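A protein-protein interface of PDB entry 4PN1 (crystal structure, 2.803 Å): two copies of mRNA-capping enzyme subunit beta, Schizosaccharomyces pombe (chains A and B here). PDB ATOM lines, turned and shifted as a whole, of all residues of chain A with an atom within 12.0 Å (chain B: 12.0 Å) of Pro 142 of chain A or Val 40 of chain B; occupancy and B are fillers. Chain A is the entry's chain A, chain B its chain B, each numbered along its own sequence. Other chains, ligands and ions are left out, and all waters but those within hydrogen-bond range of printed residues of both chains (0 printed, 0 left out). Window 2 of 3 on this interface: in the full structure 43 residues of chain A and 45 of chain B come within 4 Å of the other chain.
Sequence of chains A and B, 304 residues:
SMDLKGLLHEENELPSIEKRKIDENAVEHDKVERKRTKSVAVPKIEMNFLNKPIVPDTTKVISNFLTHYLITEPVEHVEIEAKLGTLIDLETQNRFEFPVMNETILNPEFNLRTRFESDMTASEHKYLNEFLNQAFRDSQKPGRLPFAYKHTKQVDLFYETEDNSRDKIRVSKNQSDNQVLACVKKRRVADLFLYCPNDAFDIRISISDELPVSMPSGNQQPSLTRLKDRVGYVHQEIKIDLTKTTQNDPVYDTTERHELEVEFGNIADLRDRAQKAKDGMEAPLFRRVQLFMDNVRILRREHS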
ATOM      1  N   GLN A 134     -19.777 -25.406  27.801  1.00  0.00           N
ATOM      2  CA  GLN A 134     -20.059 -24.122  27.176  1.00  0.00           C
ATOM      3  C   GLN A 134     -19.336 -24.021  25.838  1.00  0.00           C
ATOM      4  O   GLN A 134     -19.895 -23.530  24.856  1.00  0.00           O
ATOM      5  CB  GLN A 134     -19.656 -22.966  28.090  1.00  0.00           C
ATOM      6  CG  GLN A 134     -20.143 -21.615  27.594  1.00  0.00           C
ATOM      7  CD  GLN A 134     -21.637 -21.606  27.313  1.00  0.00           C
ATOM      8  OE1 GLN A 134     -22.447 -21.943  28.178  1.00  0.00           O
ATOM      9  NE2 GLN A 134     -22.007 -21.229  26.094  1.00  0.00           N
ATOM     10  N   ALA A 135     -18.095 -24.496  25.808  1.00  0.00           N
ATOM     11  CA  ALA A 135     -17.314 -24.536  24.578  1.00  0.00           C
ATOM     12  C   ALA A 135     -17.956 -25.488  23.576  1.00  0.00           C
ATOM     13  O   ALA A 135     -17.935 -25.244  22.369  1.00  0.00           O
ATOM     14  CB  ALA A 135     -15.884 -24.959  24.871  1.00  0.00           C
ATOM     15  N   PHE A 136     -18.527 -26.573  24.090  1.00  0.00           N
ATOM     16  CA  PHE A 136     -19.230 -27.550  23.263  1.00  0.00           C
ATOM     17  C   PHE A 136     -20.454 -26.930  22.597  1.00  0.00           C
ATOM     18  O   PHE A 136     -20.662 -27.090  21.393  1.00  0.00           O
ATOM     19  CB  PHE A 136     -19.645 -28.758  24.109  1.00  0.00           C
ATOM     20  CG  PHE A 136     -20.574 -29.708  23.406  1.00  0.00           C
ATOM     21  CD1 PHE A 136     -20.077 -30.688  22.564  1.00  0.00           C
ATOM     22  CD2 PHE A 136     -21.943 -29.637  23.606  1.00  0.00           C
ATOM     23  CE1 PHE A 136     -20.927 -31.568  21.921  1.00  0.00           C
ATOM     24  CE2 PHE A 136     -22.797 -30.514  22.967  1.00  0.00           C
ATOM     25  CZ  PHE A 136     -22.289 -31.481  22.123  1.00  0.00           C
ATOM     26  N   ARG A 137     -21.260 -26.225  23.384  1.00  0.00           N
ATOM     27  CA  ARG A 137     -22.474 -25.598  22.871  1.00  0.00           C
ATOM     28  C   ARG A 137     -22.170 -24.480  21.877  1.00  0.00           C
ATOM     29  O   ARG A 137     -22.854 -24.343  20.862  1.00  0.00           O
ATOM     30  CB  ARG A 137     -23.345 -25.076  24.019  1.00  0.00           C
ATOM     31  CG  ARG A 137     -24.070 -26.173  24.789  1.00  0.00           C
ATOM     32  CD  ARG A 137     -25.052 -25.604  25.804  1.00  0.00           C
ATOM     33  NE  ARG A 137     -24.377 -24.993  26.944  1.00  0.00           N
ATOM     34  CZ  ARG A 137     -24.029 -25.653  28.044  1.00  0.00           C
ATOM     35  NH1 ARG A 137     -24.292 -26.950  28.155  1.00  0.00           N
ATOM     36  NH2 ARG A 137     -23.416 -25.017  29.034  1.00  0.00           N
ATOM     37  N   ASP A 138     -21.141 -23.690  22.167  1.00  0.00           N
ATOM     38  CA  ASP A 138     -20.753 -22.583  21.297  1.00  0.00           C
ATOM     39  C   ASP A 138     -20.280 -23.053  19.923  1.00  0.00           C
ATOM     40  O   ASP A 138     -20.462 -22.357  18.926  1.00  0.00           O
ATOM     41  CB  ASP A 138     -19.657 -21.735  21.951  1.00  0.00           C
ATOM     42  CG  ASP A 138     -20.186 -20.854  23.064  1.00  0.00           C
ATOM     43  OD1 ASP A 138     -21.417 -20.659  23.138  1.00  0.00           O
ATOM     44  OD2 ASP A 138     -19.365 -20.347  23.858  1.00  0.00           O
ATOM     45  N   SER A 139     -19.673 -24.234  19.874  1.00  0.00           N
ATOM     46  CA  SER A 139     -19.099 -24.739  18.631  1.00  0.00           C
ATOM     47  C   SER A 139     -20.166 -25.258  17.674  1.00  0.00           C
ATOM     48  O   SER A 139     -19.870 -25.590  16.528  1.00  0.00           O
ATOM     49  CB  SER A 139     -18.079 -25.842  18.914  1.00  0.00           C
ATOM     50  OG  SER A 139     -18.720 -27.041  19.306  1.00  0.00           O
ATOM     51  N   GLN A 140     -21.407 -25.329  18.147  1.00  0.00           N
ATOM     52  CA  GLN A 140     -22.506 -25.800  17.313  1.00  0.00           C
ATOM     53  C   GLN A 140     -23.140 -24.644  16.549  1.00  0.00           C
ATOM     54  O   GLN A 140     -23.936 -24.852  15.633  1.00  0.00           O
ATOM     55  CB  GLN A 140     -23.557 -26.518  18.163  1.00  0.00           C
ATOM     56  CG  GLN A 140     -22.984 -27.560  19.111  1.00  0.00           C
ATOM     57  CD  GLN A 140     -22.189 -28.638  18.396  1.00  0.00           C
ATOM     58  OE1 GLN A 140     -22.407 -28.909  17.215  1.00  0.00           O
ATOM     59  NE2 GLN A 140     -21.258 -29.259  19.113  1.00  0.00           N
ATOM     60  N   LYS A 141     -22.776 -23.427  16.937  1.00  0.00           N
ATOM     61  CA  LYS A 141     -23.269 -22.218  16.290  1.00  0.00           C
ATOM     62  C   LYS A 141     -22.803 -22.150  14.836  1.00  0.00           C
ATOM     63  O   LYS A 141     -21.840 -22.819  14.462  1.00  0.00           O
ATOM     64  CB  LYS A 141     -22.792 -20.984  17.060  1.00  0.00           C
ATOM     65  CG  LYS A 141     -23.363 -20.876  18.462  1.00  0.00           C
ATOM     66  CD  LYS A 141     -22.944 -19.576  19.128  1.00  0.00           C
ATOM     67  CE  LYS A 141     -23.619 -19.412  20.480  1.00  0.00           C
ATOM     68  NZ  LYS A 141     -23.293 -18.104  21.112  1.00  0.00           N
ATOM     69  N   PRO A 142     -23.502 -21.356  14.004  1.00  0.00           N
ATOM     70  CA  PRO A 142     -23.107 -21.172  12.603  1.00  0.00           C
ATOM     71  C   PRO A 142     -21.675 -20.670  12.455  1.00  0.00           C
ATOM     72  O   PRO A 142     -21.211 -19.881  13.278  1.00  0.00           O
ATOM     73  CB  PRO A 142     -24.082 -20.102  12.111  1.00  0.00           C
ATOM     74  CG  PRO A 142     -25.297 -20.310  12.937  1.00  0.00           C
ATOM     75  CD  PRO A 142     -24.800 -20.718  14.294  1.00  0.00           C
ATOM     76  N   GLY A 143     -20.988 -21.137  11.416  1.00  0.00           N
ATOM     77  CA  GLY A 143     -19.644 -20.680  11.110  1.00  0.00           C
ATOM     78  C   GLY A 143     -18.551 -21.318  11.947  1.00  0.00           C
ATOM     79  O   GLY A 143     -17.383 -20.950  11.835  1.00  0.00           O
ATOM     80  N   ARG A 144     -18.928 -22.277  12.785  1.00  0.00           N
ATOM     81  CA  ARG A 144     -17.970 -22.944  13.660  1.00  0.00           C
ATOM     82  C   ARG A 144     -17.703 -24.380  13.218  1.00  0.00           C
ATOM     83  O   ARG A 144     -18.573 -25.033  12.640  1.00  0.00           O
ATOM     84  CB  ARG A 144     -18.478 -22.942  15.106  1.00  0.00           C
ATOM     85  CG  ARG A 144     -18.482 -21.584  15.786  1.00  0.00           C
ATOM     86  CD  ARG A 144     -17.071 -21.043  15.951  1.00  0.00           C
ATOM     87  NE  ARG A 144     -16.159 -22.052  16.483  1.00  0.00           N
ATOM     88  CZ  ARG A 144     -15.970 -22.281  17.778  1.00  0.00           C
ATOM     89  NH1 ARG A 144     -16.633 -21.573  18.682  1.00  0.00           N
ATOM     90  NH2 ARG A 144     -15.120 -23.220  18.169  1.00  0.00           N
ATOM     91  N   LEU A 145     -16.491 -24.857  13.482  1.00  0.00           N
ATOM     92  CA  LEU A 145     -16.190 -26.279  13.366  1.00  0.00           C
ATOM     93  C   LEU A 145     -16.637 -26.960  14.654  1.00  0.00           C
ATOM     94  O   LEU A 145     -16.053 -26.736  15.713  1.00  0.00           O
ATOM     95  CB  LEU A 145     -14.697 -26.508  13.124  1.00  0.00           C
ATOM     96  CG  LEU A 145     -14.213 -26.299  11.688  1.00  0.00           C
ATOM     97  CD1 LEU A 145     -12.743 -26.653  11.559  1.00  0.00           C
ATOM     98  CD2 LEU A 145     -15.044 -27.125  10.723  1.00  0.00           C
ATOM     99  N   PRO A 146     -17.685 -27.790  14.567  1.00  0.00           N
ATOM    100  CA  PRO A 146     -18.379 -28.305  15.752  1.00  0.00           C
ATOM    101  C   PRO A 146     -17.620 -29.366  16.545  1.00  0.00           C
ATOM    102  O   PRO A 146     -16.741 -30.053  16.019  1.00  0.00           O
ATOM    103  CB  PRO A 146     -19.664 -28.899  15.167  1.00  0.00           C
ATOM    104  CG  PRO A 146     -19.297 -29.282  13.783  1.00  0.00           C
ATOM    105  CD  PRO A 146     -18.314 -28.248  13.316  1.00  0.00           C
ATOM    106  N   PHE A 147     -17.978 -29.475  17.820  1.00  0.00           N
ATOM    107  CA  PHE A 147     -17.461 -30.503  18.713  1.00  0.00           C
ATOM    108  C   PHE A 147     -18.199 -31.817  18.494  1.00  0.00           C
ATOM    109  O   PHE A 147     -19.331 -31.834  18.011  1.00  0.00           O
ATOM    110  CB  PHE A 147     -17.681 -30.078  20.165  1.00  0.00           C
ATOM    111  CG  PHE A 147     -16.468 -29.494  20.833  1.00  0.00           C
ATOM    112  CD1 PHE A 147     -15.610 -30.299  21.563  1.00  0.00           C
ATOM    113  CD2 PHE A 147     -16.204 -28.136  20.761  1.00  0.00           C
ATOM    114  CE1 PHE A 147     -14.503 -29.766  22.189  1.00  0.00           C
ATOM    115  CE2 PHE A 147     -15.100 -27.597  21.388  1.00  0.00           C
ATOM    116  CZ  PHE A 147     -14.249 -28.413  22.104  1.00  0.00           C
ATOM    117  N   HIS A 235     -12.614 -32.143  18.936  1.00  0.00           N
ATOM    118  CA  HIS A 235     -12.634 -30.967  18.078  1.00  0.00           C
ATOM    119  C   HIS A 235     -11.431 -30.992  17.146  1.00  0.00           C
ATOM    120  O   HIS A 235     -10.290 -30.907  17.600  1.00  0.00           O
ATOM    121  CB  HIS A 235     -12.628 -29.689  18.917  1.00  0.00           C
ATOM    122  CG  HIS A 235     -12.750 -28.437  18.108  1.00  0.00           C
ATOM    123  ND1 HIS A 235     -11.669 -27.636  17.807  1.00  0.00           N
ATOM    124  CD2 HIS A 235     -13.826 -27.845  17.536  1.00  0.00           C
ATOM    125  CE1 HIS A 235     -12.074 -26.605  17.088  1.00  0.00           C
ATOM    126  NE2 HIS A 235     -13.379 -26.708  16.909  1.00  0.00           N
ATOM    127  N   VAL B  40     -22.747 -17.629   5.989  1.00  0.00           N
ATOM    128  CA  VAL B  40     -21.571 -17.647   6.853  1.00  0.00           C
ATOM    129  C   VAL B  40     -20.692 -18.868   6.580  1.00  0.00           C
ATOM    130  O   VAL B  40     -21.104 -20.010   6.788  1.00  0.00           O
ATOM    131  CB  VAL B  40     -21.961 -17.577   8.350  1.00  0.00           C
ATOM    132  CG1 VAL B  40     -23.111 -18.536   8.662  1.00  0.00           C
ATOM    133  CG2 VAL B  40     -20.748 -17.844   9.236  1.00  0.00           C
ATOM    134  N   ALA B  41     -19.478 -18.615   6.106  1.00  0.00           N
ATOM    135  CA  ALA B  41     -18.573 -19.683   5.698  1.00  0.00           C
ATOM    136  C   ALA B  41     -18.042 -20.488   6.880  1.00  0.00           C
ATOM    137  O   ALA B  41     -17.938 -19.981   7.998  1.00  0.00           O
ATOM    138  CB  ALA B  41     -17.418 -19.116   4.879  1.00  0.00           C
ATOM    139  N   VAL B  42     -17.715 -21.748   6.620  1.00  0.00           N
ATOM    140  CA  VAL B  42     -17.056 -22.595   7.603  1.00  0.00           C
ATOM    141  C   VAL B  42     -15.559 -22.623   7.318  1.00  0.00           C
ATOM    142  O   VAL B  42     -15.143 -22.933   6.201  1.00  0.00           O
ATOM    143  CB  VAL B  42     -17.618 -24.029   7.576  1.00  0.00           C
ATOM    144  CG1 VAL B  42     -16.655 -24.997   8.245  1.00  0.00           C
ATOM    145  CG2 VAL B  42     -18.985 -24.074   8.240  1.00  0.00           C
ATOM    146  N   PRO B  43     -14.741 -22.288   8.328  1.00  0.00           N
ATOM    147  CA  PRO B  43     -13.283 -22.244   8.171  1.00  0.00           C
ATOM    148  C   PRO B  43     -12.707 -23.613   7.828  1.00  0.00           C
ATOM    149  O   PRO B  43     -13.351 -24.631   8.078  1.00  0.00           O
ATOM    150  CB  PRO B  43     -12.796 -21.797   9.553  1.00  0.00           C
ATOM    151  CG  PRO B  43     -13.896 -22.178  10.488  1.00  0.00           C
ATOM    152  CD  PRO B  43     -15.156 -21.977   9.706  1.00  0.00           C
ATOM    153  N   LYS B  44     -11.511 -23.632   7.252  1.00  0.00           N
ATOM    154  CA  LYS B  44     -10.841 -24.886   6.939  1.00  0.00           C
ATOM    155  C   LYS B  44     -10.303 -25.493   8.230  1.00  0.00           C
ATOM    156  O   LYS B  44     -10.440 -26.693   8.472  1.00  0.00           O
ATOM    157  CB  LYS B  44      -9.706 -24.650   5.941  1.00  0.00           C
ATOM    158  CG  LYS B  44      -9.265 -25.897   5.192  1.00  0.00           C
ATOM    159  CD  LYS B  44      -8.053 -25.616   4.316  1.00  0.00           C
ATOM    160  CE  LYS B  44      -8.325 -24.491   3.327  1.00  0.00           C
ATOM    161  NZ  LYS B  44      -9.406 -24.837   2.362  1.00  0.00           N
ATOM    162  N   GLU B  46      -9.441 -24.222  12.650  1.00  0.00           N
ATOM    163  CA  GLU B  46      -9.542 -23.210  13.697  1.00  0.00           C
ATOM    164  C   GLU B  46      -8.291 -23.241  14.572  1.00  0.00           C
ATOM    165  O   GLU B  46      -7.681 -24.296  14.752  1.00  0.00           O
ATOM    166  CB  GLU B  46     -10.800 -23.421  14.540  1.00  0.00           C
ATOM    167  CG  GLU B  46     -12.099 -23.248  13.765  1.00  0.00           C
ATOM    168  CD  GLU B  46     -13.329 -23.350  14.648  1.00  0.00           C
ATOM    169  OE1 GLU B  46     -13.321 -24.167  15.594  1.00  0.00           O
ATOM    170  OE2 GLU B  46     -14.305 -22.611  14.398  1.00  0.00           O
ATOM    171  N   PHE B  49     -10.044 -24.703  20.118  1.00  0.00           N
ATOM    172  CA  PHE B  49     -11.456 -25.068  20.245  1.00  0.00           C
ATOM    173  C   PHE B  49     -12.379 -23.908  20.636  1.00  0.00           C
ATOM    174  O   PHE B  49     -13.602 -24.033  20.560  1.00  0.00           O
ATOM    175  CB  PHE B  49     -11.667 -26.307  21.140  1.00  0.00           C
ATOM    176  CG  PHE B  49     -11.288 -26.113  22.589  1.00  0.00           C
ATOM    177  CD1 PHE B  49     -12.054 -25.316  23.429  1.00  0.00           C
ATOM    178  CD2 PHE B  49     -10.195 -26.777  23.123  1.00  0.00           C
ATOM    179  CE1 PHE B  49     -11.712 -25.155  24.761  1.00  0.00           C
ATOM    180  CE2 PHE B  49      -9.851 -26.622  24.455  1.00  0.00           C
ATOM    181  CZ  PHE B  49     -10.613 -25.811  25.274  1.00  0.00           C
ATOM    182  N   LEU B  50     -11.796 -22.788  21.050  1.00  0.00           N
ATOM    183  CA  LEU B  50     -12.579 -21.589  21.333  1.00  0.00           C
ATOM    184  C   LEU B  50     -12.719 -20.726  20.086  1.00  0.00           C
ATOM    185  O   LEU B  50     -13.611 -19.878  20.003  1.00  0.00           O
ATOM    186  CB  LEU B  50     -11.944 -20.764  22.456  1.00  0.00           C
ATOM    187  CG  LEU B  50     -11.993 -21.314  23.881  1.00  0.00           C
ATOM    188  CD1 LEU B  50     -11.670 -20.211  24.880  1.00  0.00           C
ATOM    189  CD2 LEU B  50     -13.345 -21.937  24.181  1.00  0.00           C
ATOM    190  N   ASN B  51     -11.833 -20.955  19.120  1.00  0.00           N
ATOM    191  CA  ASN B  51     -11.746 -20.133  17.914  1.00  0.00           C
ATOM    192  C   ASN B  51     -11.522 -18.654  18.246  1.00  0.00           C
ATOM    193  O   ASN B  51     -12.070 -17.759  17.601  1.00  0.00           O
ATOM    194  CB  ASN B  51     -12.967 -20.340  17.010  1.00  0.00           C
ATOM    195  CG  ASN B  51     -12.778 -19.744  15.627  1.00  0.00           C
ATOM    196  OD1 ASN B  51     -11.947 -20.207  14.845  1.00  0.00           O
ATOM    197  ND2 ASN B  51     -13.555 -18.711  15.319  1.00  0.00           N
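No position is printed for both chains.
Of the 14 pairs that touch across the chains among the printed residues, none has its exchanged pair printed and touching as well.
NE2 of His 235 of chain A lies within hydrogen-bond range of O of Leu 145 of chain A, at 2.9 Å.
The side-chain amide nitrogen of Gln 140 of chain A sits at hydrogen-bond distance from the backbone carbonyl oxygen of Phe 147 of chain A.
The side-chain hydroxyl of Ser 139 of chain A sits at hydrogen-bond distance from the backbone NH of Phe 147 of chain A.
The side-chain carboxylate of Glu 46 of chain B sits close to the side-chain amide oxygen of Asn 51 of chain B.
The side-chain carboxylate (OE2) of Glu 46 of chain B is in hydrogen-bond range of the backbone NH (N) of Leu 145 of chain A (3.3 Å).
The guanidinium group (NE) of Arg 144 of chain A lies within salt-bridge range of the side-chain carboxylate (OE2) of Glu 46 of chain B (2.8 Å).
The guanidinium group of Arg 144 of chain A is in hydrogen-bond range of the backbone carbonyl oxygen of Phe 49 of chain B (2.9 Å).
A ring nitrogen (NE2) of His 235 of chain A sits at hydrogen-bond distance from the side-chain carboxylate (OE1) of Glu 46 of chain B.
Of the 9 printed residues of chain B, 9 touch a printed residue of chain A.
Along chain B the printed residues that touch a printed residue of chain A span positions 40 to 51.
Of the 15 printed residues of chain A, 6 touch a printed residue of chain B.
Gln 140 of chain A touches none of the printed residues of chain B.
No residue of chain B comes within 4 Å of Lys 141 of chain A.
Val 40 of chain B touches two residues of chain A.
Of chain A, only Gly 143 (3.6 Å) comes within 4 Å of Ala 41 of chain B.
Printed residues of chain A within 4 Å of Val 42 of chain B: Leu 145 (3.6 Å).
Of the printed residues of chain A, Pro 43 of chain B touches Gly 143 (3.2 Å).
Of the printed residues of chain A, Leu 50 of chain B touches Arg 144.
The nearest residue of chain A that does not touch Val 40 of chain B is Arg 144 of chain A (6.0 Å).
Among the printed residues, pairs that only touch across the chains: Gly 143 of chain A with Pro 43 of chain B (3.2 Å), Phe 147 of chain A with Phe 49 of chain B (3.5 Å), His 235 of chain A with Phe 49 of chain B (3.5 Å), Gly 143 of chain A with Val 40 of chain B (3.6 Å), Gly 143 of chain A with Ala 41 of chain B (3.6 Å), Leu 145 of chain A with Val 42 of chain B (3.6 Å), Arg 144 of chain A with Asn 51 of chain B (3.7 Å), Arg 144 of chain A with Leu 50 of chain B (3.7 Å), Leu 145 of chain A with Lys 44 of chain B (3.9 Å) and Pro 142 of chain A with Val 40 of chain B (3.9 Å).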
